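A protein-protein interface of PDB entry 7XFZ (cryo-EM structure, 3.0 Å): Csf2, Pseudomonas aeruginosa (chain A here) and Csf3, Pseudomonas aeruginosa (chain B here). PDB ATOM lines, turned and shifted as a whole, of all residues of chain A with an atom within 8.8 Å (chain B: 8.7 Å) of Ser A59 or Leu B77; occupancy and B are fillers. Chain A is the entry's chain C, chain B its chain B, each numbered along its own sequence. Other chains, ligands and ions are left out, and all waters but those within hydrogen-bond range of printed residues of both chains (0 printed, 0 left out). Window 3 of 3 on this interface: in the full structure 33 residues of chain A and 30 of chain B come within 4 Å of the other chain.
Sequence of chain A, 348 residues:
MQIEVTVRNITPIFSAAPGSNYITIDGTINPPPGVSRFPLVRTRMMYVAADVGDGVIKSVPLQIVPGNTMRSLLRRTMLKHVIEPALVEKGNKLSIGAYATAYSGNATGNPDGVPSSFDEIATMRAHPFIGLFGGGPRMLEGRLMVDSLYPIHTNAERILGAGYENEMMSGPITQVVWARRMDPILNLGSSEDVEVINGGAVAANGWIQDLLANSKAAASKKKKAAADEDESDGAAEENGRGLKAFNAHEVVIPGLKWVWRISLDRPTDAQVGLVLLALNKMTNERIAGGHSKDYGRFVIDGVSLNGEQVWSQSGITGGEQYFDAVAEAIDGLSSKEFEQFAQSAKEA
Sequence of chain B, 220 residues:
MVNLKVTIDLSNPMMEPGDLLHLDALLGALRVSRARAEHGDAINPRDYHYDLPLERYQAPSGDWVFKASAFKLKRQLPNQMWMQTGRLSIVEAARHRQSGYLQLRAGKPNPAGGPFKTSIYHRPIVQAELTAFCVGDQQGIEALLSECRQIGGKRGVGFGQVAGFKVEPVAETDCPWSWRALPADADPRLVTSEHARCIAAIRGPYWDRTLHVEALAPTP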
ATOM      1  N   MET A  45      12.177 -11.946 -19.874  1.00  0.00           N
ATOM      2  CA  MET A  45      13.255 -11.450 -19.035  1.00  0.00           C
ATOM      3  C   MET A  45      12.697 -11.068 -17.674  1.00  0.00           C
ATOM      4  O   MET A  45      11.555 -10.618 -17.559  1.00  0.00           O
ATOM      5  CB  MET A  45      13.957 -10.275 -19.728  1.00  0.00           C
ATOM      6  CG  MET A  45      14.698  -9.308 -18.842  1.00  0.00           C
ATOM      7  SD  MET A  45      13.580  -8.011 -18.285  1.00  0.00           S
ATOM      8  CE  MET A  45      14.685  -7.019 -17.314  1.00  0.00           C
ATOM      9  N   MET A  46      13.514 -11.265 -16.640  1.00  0.00           N
ATOM     10  CA  MET A  46      13.140 -10.946 -15.271  1.00  0.00           C
ATOM     11  C   MET A  46      14.300 -10.245 -14.577  1.00  0.00           C
ATOM     12  O   MET A  46      15.465 -10.418 -14.942  1.00  0.00           O
ATOM     13  CB  MET A  46      12.726 -12.208 -14.503  1.00  0.00           C
ATOM     14  CG  MET A  46      13.887 -12.993 -13.927  1.00  0.00           C
ATOM     15  SD  MET A  46      13.383 -14.376 -12.894  1.00  0.00           S
ATOM     16  CE  MET A  46      11.890 -13.724 -12.164  1.00  0.00           C
ATOM     17  N   TYR A  47      13.966  -9.442 -13.569  1.00  0.00           N
ATOM     18  CA  TYR A  47      14.962  -8.749 -12.761  1.00  0.00           C
ATOM     19  C   TYR A  47      15.370  -9.615 -11.576  1.00  0.00           C
ATOM     20  O   TYR A  47      14.513 -10.162 -10.876  1.00  0.00           O
ATOM     21  CB  TYR A  47      14.428  -7.407 -12.261  1.00  0.00           C
ATOM     22  CG  TYR A  47      14.332  -6.340 -13.323  1.00  0.00           C
ATOM     23  CD1 TYR A  47      15.474  -5.769 -13.863  1.00  0.00           C
ATOM     24  CD2 TYR A  47      13.100  -5.895 -13.780  1.00  0.00           C
ATOM     25  CE1 TYR A  47      15.393  -4.791 -14.827  1.00  0.00           C
ATOM     26  CE2 TYR A  47      13.009  -4.919 -14.747  1.00  0.00           C
ATOM     27  CZ  TYR A  47      14.158  -4.371 -15.269  1.00  0.00           C
ATOM     28  OH  TYR A  47      14.071  -3.398 -16.235  1.00  0.00           O
ATOM     29  N   VAL A  48      16.675  -9.729 -11.353  1.00  0.00           N
ATOM     30  CA  VAL A  48      17.228 -10.496 -10.245  1.00  0.00           C
ATOM     31  C   VAL A  48      18.219  -9.619  -9.497  1.00  0.00           C
ATOM     32  O   VAL A  48      18.766  -8.666 -10.059  1.00  0.00           O
ATOM     33  CB  VAL A  48      17.908 -11.796 -10.724  1.00  0.00           C
ATOM     34  CG1 VAL A  48      16.908 -12.701 -11.421  1.00  0.00           C
ATOM     35  CG2 VAL A  48      19.077 -11.480 -11.645  1.00  0.00           C
ATOM     36  N   ALA A  49      18.444  -9.941  -8.226  1.00  0.00           N
ATOM     37  CA  ALA A  49      19.400  -9.217  -7.392  1.00  0.00           C
ATOM     38  C   ALA A  49      20.722  -9.969  -7.423  1.00  0.00           C
ATOM     39  O   ALA A  49      20.869 -11.015  -6.786  1.00  0.00           O
ATOM     40  CB  ALA A  49      18.874  -9.073  -5.969  1.00  0.00           C
ATOM     41  N   ALA A  50      21.689  -9.440  -8.163  1.00  0.00           N
ATOM     42  CA  ALA A  50      23.004 -10.054  -8.294  1.00  0.00           C
ATOM     43  C   ALA A  50      24.008  -9.284  -7.454  1.00  0.00           C
ATOM     44  O   ALA A  50      24.238  -8.093  -7.689  1.00  0.00           O
ATOM     45  CB  ALA A  50      23.457 -10.086  -9.754  1.00  0.00           C
ATOM     46  N   ASP A  51      24.608  -9.964  -6.486  1.00  0.00           N
ATOM     47  CA  ASP A  51      25.607  -9.359  -5.617  1.00  0.00           C
ATOM     48  C   ASP A  51      26.955  -9.391  -6.325  1.00  0.00           C
ATOM     49  O   ASP A  51      27.413 -10.455  -6.755  1.00  0.00           O
ATOM     50  CB  ASP A  51      25.662 -10.089  -4.272  1.00  0.00           C
ATOM     51  CG  ASP A  51      26.621  -9.444  -3.282  1.00  0.00           C
ATOM     52  OD1 ASP A  51      27.242  -8.412  -3.617  1.00  0.00           O
ATOM     53  OD2 ASP A  51      26.758  -9.977  -2.160  1.00  0.00           O
ATOM     54  N   VAL A  52      27.583  -8.226  -6.448  1.00  0.00           N
ATOM     55  CA  VAL A  52      28.902  -8.117  -7.056  1.00  0.00           C
ATOM     56  C   VAL A  52      29.912  -7.877  -5.944  1.00  0.00           C
ATOM     57  O   VAL A  52      29.535  -7.710  -4.778  1.00  0.00           O
ATOM     58  CB  VAL A  52      28.951  -6.998  -8.113  1.00  0.00           C
ATOM     59  CG1 VAL A  52      27.936  -7.268  -9.213  1.00  0.00           C
ATOM     60  CG2 VAL A  52      28.699  -5.647  -7.469  1.00  0.00           C
ATOM     61  N   VAL A  56      26.883  -4.144  -3.604  1.00  0.00           N
ATOM     62  CA  VAL A  56      25.729  -3.271  -3.790  1.00  0.00           C
ATOM     63  C   VAL A  56      24.458  -4.087  -4.007  1.00  0.00           C
ATOM     64  O   VAL A  56      23.349  -3.594  -3.768  1.00  0.00           O
ATOM     65  CB  VAL A  56      26.003  -2.298  -4.956  1.00  0.00           C
ATOM     66  CG1 VAL A  56      26.308  -3.066  -6.234  1.00  0.00           C
ATOM     67  CG2 VAL A  56      24.848  -1.321  -5.153  1.00  0.00           C
ATOM     68  N   ILE A  57      24.600  -5.338  -4.453  1.00  0.00           N
ATOM     69  CA  ILE A  57      23.507  -6.279  -4.714  1.00  0.00           C
ATOM     70  C   ILE A  57      22.398  -5.611  -5.528  1.00  0.00           C
ATOM     71  O   ILE A  57      21.204  -5.826  -5.293  1.00  0.00           O
ATOM     72  CB  ILE A  57      23.001  -6.927  -3.401  1.00  0.00           C
ATOM     73  CG1 ILE A  57      22.322  -8.270  -3.687  1.00  0.00           C
ATOM     74  CG2 ILE A  57      22.113  -6.009  -2.544  1.00  0.00           C
ATOM     75  CD1 ILE A  57      21.752  -8.939  -2.462  1.00  0.00           C
ATOM     76  N   LYS A  58      22.795  -4.838  -6.536  1.00  0.00           N
ATOM     77  CA  LYS A  58      21.845  -4.136  -7.386  1.00  0.00           C
ATOM     78  C   LYS A  58      21.041  -5.114  -8.242  1.00  0.00           C
ATOM     79  O   LYS A  58      21.261  -6.329  -8.224  1.00  0.00           O
ATOM     80  CB  LYS A  58      22.573  -3.136  -8.280  1.00  0.00           C
ATOM     81  CG  LYS A  58      23.364  -3.784  -9.403  1.00  0.00           C
ATOM     82  CD  LYS A  58      24.377  -2.819  -9.991  1.00  0.00           C
ATOM     83  CE  LYS A  58      25.600  -3.556 -10.512  1.00  0.00           C
ATOM     84  NZ  LYS A  58      26.252  -4.372  -9.450  1.00  0.00           N
ATOM     85  N   SER A  59      20.094  -4.564  -8.999  1.00  0.00           N
ATOM     86  CA  SER A  59      19.233  -5.377  -9.848  1.00  0.00           C
ATOM     87  C   SER A  59      19.740  -5.380 -11.284  1.00  0.00           C
ATOM     88  O   SER A  59      20.074  -4.329 -11.839  1.00  0.00           O
ATOM     89  CB  SER A  59      17.801  -4.855  -9.804  1.00  0.00           C
ATOM     90  OG  SER A  59      17.632  -3.774 -10.700  1.00  0.00           O
ATOM     91  N   VAL A  60      19.782  -6.562 -11.892  1.00  0.00           N
ATOM     92  CA  VAL A  60      20.286  -6.720 -13.254  1.00  0.00           C
ATOM     93  C   VAL A  60      19.289  -7.538 -14.068  1.00  0.00           C
ATOM     94  O   VAL A  60      18.530  -8.331 -13.495  1.00  0.00           O
ATOM     95  CB  VAL A  60      21.673  -7.378 -13.258  1.00  0.00           C
ATOM     96  CG1 VAL A  60      22.713  -6.434 -12.684  1.00  0.00           C
ATOM     97  CG2 VAL A  60      21.640  -8.670 -12.476  1.00  0.00           C
ATOM     98  N   PRO A  61      19.249  -7.379 -15.389  1.00  0.00           N
ATOM     99  CA  PRO A  61      18.330  -8.182 -16.203  1.00  0.00           C
ATOM    100  C   PRO A  61      18.916  -9.538 -16.566  1.00  0.00           C
ATOM    101  O   PRO A  61      20.105  -9.666 -16.866  1.00  0.00           O
ATOM    102  CB  PRO A  61      18.132  -7.316 -17.451  1.00  0.00           C
ATOM    103  CG  PRO A  61      19.407  -6.576 -17.584  1.00  0.00           C
ATOM    104  CD  PRO A  61      19.947  -6.359 -16.191  1.00  0.00           C
ATOM    105  N   LEU A  62      18.060 -10.558 -16.544  1.00  0.00           N
ATOM    106  CA  LEU A  62      18.447 -11.918 -16.896  1.00  0.00           C
ATOM    107  C   LEU A  62      17.410 -12.508 -17.837  1.00  0.00           C
ATOM    108  O   LEU A  62      16.207 -12.417 -17.575  1.00  0.00           O
ATOM    109  CB  LEU A  62      18.593 -12.792 -15.646  1.00  0.00           C
ATOM    110  CG  LEU A  62      19.248 -14.163 -15.828  1.00  0.00           C
ATOM    111  CD1 LEU A  62      20.693 -14.028 -16.271  1.00  0.00           C
ATOM    112  CD2 LEU A  62      19.153 -14.970 -14.549  1.00  0.00           C
ATOM    113  N   ASN A 155      25.214 -12.524 -14.512  1.00  0.00           N
ATOM    114  CA  ASN A 155      24.027 -11.982 -13.859  1.00  0.00           C
ATOM    115  C   ASN A 155      23.283 -13.052 -13.075  1.00  0.00           C
ATOM    116  O   ASN A 155      22.369 -12.735 -12.306  1.00  0.00           O
ATOM    117  CB  ASN A 155      23.102 -11.337 -14.889  1.00  0.00           C
ATOM    118  CG  ASN A 155      23.603  -9.989 -15.357  1.00  0.00           C
ATOM    119  OD1 ASN A 155      24.671  -9.538 -14.949  1.00  0.00           O
ATOM    120  ND2 ASN A 155      22.830  -9.335 -16.211  1.00  0.00           N
ATOM    121  N   ARG A 158      23.787 -15.248  -8.368  1.00  0.00           N
ATOM    122  CA  ARG A 158      23.016 -15.454  -7.149  1.00  0.00           C
ATOM    123  C   ARG A 158      22.239 -16.763  -7.201  1.00  0.00           C
ATOM    124  O   ARG A 158      22.181 -17.499  -6.210  1.00  0.00           O
ATOM    125  CB  ARG A 158      22.078 -14.271  -6.922  1.00  0.00           C
ATOM    126  CG  ARG A 158      21.387 -14.270  -5.576  1.00  0.00           C
ATOM    127  CD  ARG A 158      22.111 -13.356  -4.609  1.00  0.00           C
ATOM    128  NE  ARG A 158      21.583 -13.454  -3.255  1.00  0.00           N
ATOM    129  CZ  ARG A 158      20.484 -12.845  -2.834  1.00  0.00           C
ATOM    130  NH1 ARG A 158      19.759 -12.090  -3.641  1.00  0.00           N
ATOM    131  NH2 ARG A 158      20.104 -12.994  -1.568  1.00  0.00           N
ATOM    132  N   LEU B  10      16.455 -15.523   0.827  1.00  0.00           N
ATOM    133  CA  LEU B  10      16.105 -16.278  -0.368  1.00  0.00           C
ATOM    134  C   LEU B  10      16.907 -15.778  -1.563  1.00  0.00           C
ATOM    135  O   LEU B  10      17.143 -14.577  -1.708  1.00  0.00           O
ATOM    136  CB  LEU B  10      14.596 -16.214  -0.650  1.00  0.00           C
ATOM    137  CG  LEU B  10      13.750 -14.945  -0.530  1.00  0.00           C
ATOM    138  CD1 LEU B  10      14.094 -13.916  -1.584  1.00  0.00           C
ATOM    139  CD2 LEU B  10      12.280 -15.298  -0.602  1.00  0.00           C
ATOM    140  N   ASN B  12      16.056 -16.159  -4.777  1.00  0.00           N
ATOM    141  CA  ASN B  12      15.153 -16.265  -5.912  1.00  0.00           C
ATOM    142  C   ASN B  12      13.930 -15.419  -5.618  1.00  0.00           C
ATOM    143  O   ASN B  12      13.455 -15.407  -4.477  1.00  0.00           O
ATOM    144  CB  ASN B  12      14.747 -17.726  -6.148  1.00  0.00           C
ATOM    145  CG  ASN B  12      14.476 -18.031  -7.597  1.00  0.00           C
ATOM    146  OD1 ASN B  12      13.533 -18.747  -7.923  1.00  0.00           O
ATOM    147  ND2 ASN B  12      15.311 -17.501  -8.479  1.00  0.00           N
ATOM    148  N   PRO B  13      13.410 -14.689  -6.601  1.00  0.00           N
ATOM    149  CA  PRO B  13      12.140 -13.987  -6.391  1.00  0.00           C
ATOM    150  C   PRO B  13      11.031 -14.969  -6.049  1.00  0.00           C
ATOM    151  O   PRO B  13      10.968 -16.076  -6.586  1.00  0.00           O
ATOM    152  CB  PRO B  13      11.892 -13.294  -7.734  1.00  0.00           C
ATOM    153  CG  PRO B  13      13.246 -13.135  -8.320  1.00  0.00           C
ATOM    154  CD  PRO B  13      14.018 -14.348  -7.897  1.00  0.00           C
ATOM    155  N   MET B  14      10.153 -14.555  -5.141  1.00  0.00           N
ATOM    156  CA  MET B  14       9.062 -15.395  -4.679  1.00  0.00           C
ATOM    157  C   MET B  14       7.735 -14.711  -4.960  1.00  0.00           C
ATOM    158  O   MET B  14       7.666 -13.490  -5.106  1.00  0.00           O
ATOM    159  CB  MET B  14       9.180 -15.699  -3.183  1.00  0.00           C
ATOM    160  CG  MET B  14       8.824 -14.534  -2.284  1.00  0.00           C
ATOM    161  SD  MET B  14       8.395 -15.050  -0.614  1.00  0.00           S
ATOM    162  CE  MET B  14       7.879 -13.491   0.088  1.00  0.00           C
ATOM    163  N   LYS B  74      11.509  -6.909   3.622  1.00  0.00           N
ATOM    164  CA  LYS B  74      12.448  -5.818   3.387  1.00  0.00           C
ATOM    165  C   LYS B  74      12.873  -5.907   1.926  1.00  0.00           C
ATOM    166  O   LYS B  74      13.761  -6.690   1.578  1.00  0.00           O
ATOM    167  CB  LYS B  74      13.645  -5.908   4.332  1.00  0.00           C
ATOM    168  CG  LYS B  74      14.771  -4.932   4.028  1.00  0.00           C
ATOM    169  CD  LYS B  74      16.013  -5.648   3.519  1.00  0.00           C
ATOM    170  CE  LYS B  74      17.027  -5.852   4.633  1.00  0.00           C
ATOM    171  NZ  LYS B  74      17.898  -7.035   4.394  1.00  0.00           N
ATOM    172  N   ARG B  75      12.234  -5.107   1.077  1.00  0.00           N
ATOM    173  CA  ARG B  75      12.377  -5.250  -0.364  1.00  0.00           C
ATOM    174  C   ARG B  75      13.770  -4.850  -0.833  1.00  0.00           C
ATOM    175  O   ARG B  75      14.340  -3.859  -0.370  1.00  0.00           O
ATOM    176  CB  ARG B  75      11.329  -4.404  -1.084  1.00  0.00           C
ATOM    177  CG  ARG B  75      10.003  -5.104  -1.288  1.00  0.00           C
ATOM    178  CD  ARG B  75       8.849  -4.163  -1.027  1.00  0.00           C
ATOM    179  NE  ARG B  75       7.605  -4.650  -1.608  1.00  0.00           N
ATOM    180  CZ  ARG B  75       6.557  -5.051  -0.904  1.00  0.00           C
ATOM    181  NH1 ARG B  75       6.567  -5.038   0.419  1.00  0.00           N
ATOM    182  NH2 ARG B  75       5.472  -5.476  -1.541  1.00  0.00           N
ATOM    183  N   GLN B  76      14.312  -5.632  -1.770  1.00  0.00           N
ATOM    184  CA  GLN B  76      15.598  -5.341  -2.384  1.00  0.00           C
ATOM    185  C   GLN B  76      15.498  -5.097  -3.882  1.00  0.00           C
ATOM    186  O   GLN B  76      16.508  -4.750  -4.504  1.00  0.00           O
ATOM    187  CB  GLN B  76      16.587  -6.486  -2.133  1.00  0.00           C
ATOM    188  CG  GLN B  76      16.596  -7.005  -0.712  1.00  0.00           C
ATOM    189  CD  GLN B  76      17.473  -8.227  -0.552  1.00  0.00           C
ATOM    190  OE1 GLN B  76      17.387  -9.171  -1.335  1.00  0.00           O
ATOM    191  NE2 GLN B  76      18.326  -8.213   0.464  1.00  0.00           N
ATOM    192  N   LEU B  77      14.322  -5.270  -4.474  1.00  0.00           N
ATOM    193  CA  LEU B  77      14.094  -5.134  -5.901  1.00  0.00           C
ATOM    194  C   LEU B  77      12.856  -4.285  -6.141  1.00  0.00           C
ATOM    195  O   LEU B  77      11.993  -4.181  -5.264  1.00  0.00           O
ATOM    196  CB  LEU B  77      13.895  -6.507  -6.561  1.00  0.00           C
ATOM    197  CG  LEU B  77      15.096  -7.435  -6.733  1.00  0.00           C
ATOM    198  CD1 LEU B  77      14.756  -8.550  -7.702  1.00  0.00           C
ATOM    199  CD2 LEU B  77      16.300  -6.665  -7.210  1.00  0.00           C
ATOM    200  N   PRO B  78      12.749  -3.658  -7.308  1.00  0.00           N
ATOM    201  CA  PRO B  78      11.476  -3.039  -7.688  1.00  0.00           C
ATOM    202  C   PRO B  78      10.414  -4.096  -7.946  1.00  0.00           C
ATOM    203  O   PRO B  78      10.714  -5.245  -8.278  1.00  0.00           O
ATOM    204  CB  PRO B  78      11.818  -2.266  -8.966  1.00  0.00           C
ATOM    205  CG  PRO B  78      13.067  -2.891  -9.472  1.00  0.00           C
ATOM    206  CD  PRO B  78      13.820  -3.354  -8.269  1.00  0.00           C
ATOM    207  N   ASN B  79       9.157  -3.696  -7.779  1.00  0.00           N
ATOM    208  CA  ASN B  79       8.051  -4.628  -7.946  1.00  0.00           C
ATOM    209  C   ASN B  79       7.809  -4.921  -9.421  1.00  0.00           C
ATOM    210  O   ASN B  79       7.686  -4.008 -10.241  1.00  0.00           O
ATOM    211  CB  ASN B  79       6.781  -4.065  -7.310  1.00  0.00           C
ATOM    212  CG  ASN B  79       6.806  -4.133  -5.798  1.00  0.00           C
ATOM    213  OD1 ASN B  79       7.213  -5.136  -5.216  1.00  0.00           O
ATOM    214  ND2 ASN B  79       6.365  -3.063  -5.152  1.00  0.00           N
ATOM    215  N   GLN B  80       7.727  -6.207  -9.753  1.00  0.00           N
ATOM    216  CA  GLN B  80       7.500  -6.660 -11.117  1.00  0.00           C
ATOM    217  C   GLN B  80       6.349  -7.653 -11.129  1.00  0.00           C
ATOM    218  O   GLN B  80       5.927  -8.155 -10.086  1.00  0.00           O
ATOM    219  CB  GLN B  80       8.752  -7.305 -11.718  1.00  0.00           C
ATOM    220  CG  GLN B  80       9.559  -8.117 -10.733  1.00  0.00           C
ATOM    221  CD  GLN B  80      10.740  -8.798 -11.380  1.00  0.00           C
ATOM    222  OE1 GLN B  80      10.745  -9.044 -12.584  1.00  0.00           O
ATOM    223  NE2 GLN B  80      11.750  -9.112 -10.582  1.00  0.00           N
ATOM    224  N   ILE B 125       5.653 -10.649  -8.192  1.00  0.00           N
ATOM    225  CA  ILE B 125       6.759 -11.351  -7.551  1.00  0.00           C
ATOM    226  C   ILE B 125       7.622 -10.335  -6.817  1.00  0.00           C
ATOM    227  O   ILE B 125       7.637  -9.151  -7.175  1.00  0.00           O
ATOM    228  CB  ILE B 125       7.599 -12.154  -8.561  1.00  0.00           C
ATOM    229  CG1 ILE B 125       7.990 -11.295  -9.760  1.00  0.00           C
ATOM    230  CG2 ILE B 125       6.850 -13.378  -9.026  1.00  0.00           C
ATOM    231  CD1 ILE B 125       8.961 -11.983 -10.685  1.00  0.00           C
ATOM    232  N   VAL B 126       8.328 -10.795  -5.787  1.00  0.00           N
ATOM    233  CA  VAL B 126       9.129  -9.930  -4.934  1.00  0.00           C
ATOM    234  C   VAL B 126      10.374 -10.685  -4.483  1.00  0.00           C
ATOM    235  O   VAL B 126      10.404 -11.915  -4.427  1.00  0.00           O
ATOM    236  CB  VAL B 126       8.319  -9.421  -3.720  1.00  0.00           C
ATOM    237  CG1 VAL B 126       8.130 -10.525  -2.698  1.00  0.00           C
ATOM    238  CG2 VAL B 126       8.979  -8.206  -3.094  1.00  0.00           C
ATOM    239  N   GLN B 127      11.419  -9.922  -4.172  1.00  0.00           N
ATOM    240  CA  GLN B 127      12.647 -10.454  -3.587  1.00  0.00           C
ATOM    241  C   GLN B 127      12.956  -9.609  -2.360  1.00  0.00           C
ATOM    242  O   GLN B 127      13.148  -8.396  -2.482  1.00  0.00           O
ATOM    243  CB  GLN B 127      13.800 -10.415  -4.585  1.00  0.00           C
ATOM    244  CG  GLN B 127      15.159 -10.684  -3.982  1.00  0.00           C
ATOM    245  CD  GLN B 127      15.860 -11.844  -4.646  1.00  0.00           C
ATOM    246  OE1 GLN B 127      15.976 -11.893  -5.868  1.00  0.00           O
ATOM    247  NE2 GLN B 127      16.335 -12.786  -3.845  1.00  0.00           N
ATOM    248  N   ALA B 128      13.000 -10.231  -1.185  1.00  0.00           N
ATOM    249  CA  ALA B 128      13.082  -9.446   0.038  1.00  0.00           C
ATOM    250  C   ALA B 128      13.676 -10.274   1.168  1.00  0.00           C
ATOM    251  O   ALA B 128      13.786 -11.499   1.082  1.00  0.00           O
ATOM    252  CB  ALA B 128      11.704  -8.916   0.443  1.00  0.00           C
ATOM    253  N   GLU B 129      14.073  -9.567   2.224  1.00  0.00           N
ATOM    254  CA  GLU B 129      14.357 -10.179   3.514  1.00  0.00           C
ATOM    255  C   GLU B 129      13.054 -10.408   4.265  1.00  0.00           C
ATOM    256  O   GLU B 129      12.185  -9.533   4.305  1.00  0.00           O
ATOM    257  CB  GLU B 129      15.265  -9.276   4.344  1.00  0.00           C
ATOM    258  CG  GLU B 129      16.103  -9.977   5.393  1.00  0.00           C
ATOM    259  CD  GLU B 129      17.512 -10.247   4.921  1.00  0.00           C
ATOM    260  OE1 GLU B 129      18.289 -10.850   5.691  1.00  0.00           O
ATOM    261  OE2 GLU B 129      17.845  -9.853   3.784  1.00  0.00           O
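NH2 of Arg A158 lies within hydrogen-bond range of O of Leu B10 (3.4 Å).
The side-chain amide nitrogen of Gln B80 is in hydrogen-bond range of the backbone carbonyl oxygen of Tyr A47 (3.0 Å).
The side-chain amide nitrogen (NE2) of Gln B127 sits close to the guanidinium group (NH1) of Arg A158 (3.5 Å).
The backbone carbonyl oxygen (O) of Leu B10 lies within hydrogen-bond range of the side-chain amide nitrogen (NE2) of Gln B127 (2.9 Å).
The backbone NH (N) of Gln B76 sits at hydrogen-bond distance from the backbone carbonyl oxygen (O) of Gln B127, 3.1 Å away.
The backbone carbonyl oxygen (O) of Gln B80 lies within hydrogen-bond range of the backbone NH (N) of Ile B125.
O of Met A46 lies within hydrogen-bond range of N of Leu A62 (3.1 Å).
Among the printed residues, merely in contact across the chains: Ser A59 with Leu B77, Tyr A47 with Leu B77, Met A46 with Ile B125, Ala A49 with Leu B77 and Ala A49 with Gln B127.
Met A45 touches none of the printed residues of chain B.
Of the printed residues of chain B, Tyr A47 touches Leu B77 and Gln B80.
Printed residues of chain B within 4 Å of Ala A49: Leu B77 (3.7 Å) and Gln B127 (3.9 Å).
Of chain B, only Leu B77 (3.5 Å) comes within 4 Å of Ser A59.
Val A60 touches none of the printed residues of chain B.
Asn A155 touches none of the printed residues of chain B.
Leu B77 touches just these residues of chain A: Tyr A47 (3.6 Å), Ala A49 (3.7 Å) and Ser A59 (3.5 Å).
No residue of chain A comes within 4 Å of Pro B78.
Of the printed residues of chain A, Ile B125 touches Met A46.
The nearest residue of chain A that does not touch Leu B77 is Val A48 (4.04 Å).
The nearest printed residue of chain B that does not touch Ala A49 is Gln B76 (4.9 Å).
Printed residues of chain B that touch a printed residue of chain A: Leu B10, Leu B77, Gln B80, Ile B125 and Gln B127.
Hydrophobic or aromatic side chains of chain B within 4 Å of the printed part of chain A: Leu B77 and Ile B125.
Hydrophobic or aromatic side chains of chain A within 4 Å of the printed part of chain B: Met A46, Tyr A47 and Ala A49.
Along chain A the printed residues that touch a printed residue of chain B span positions 46 to 158.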
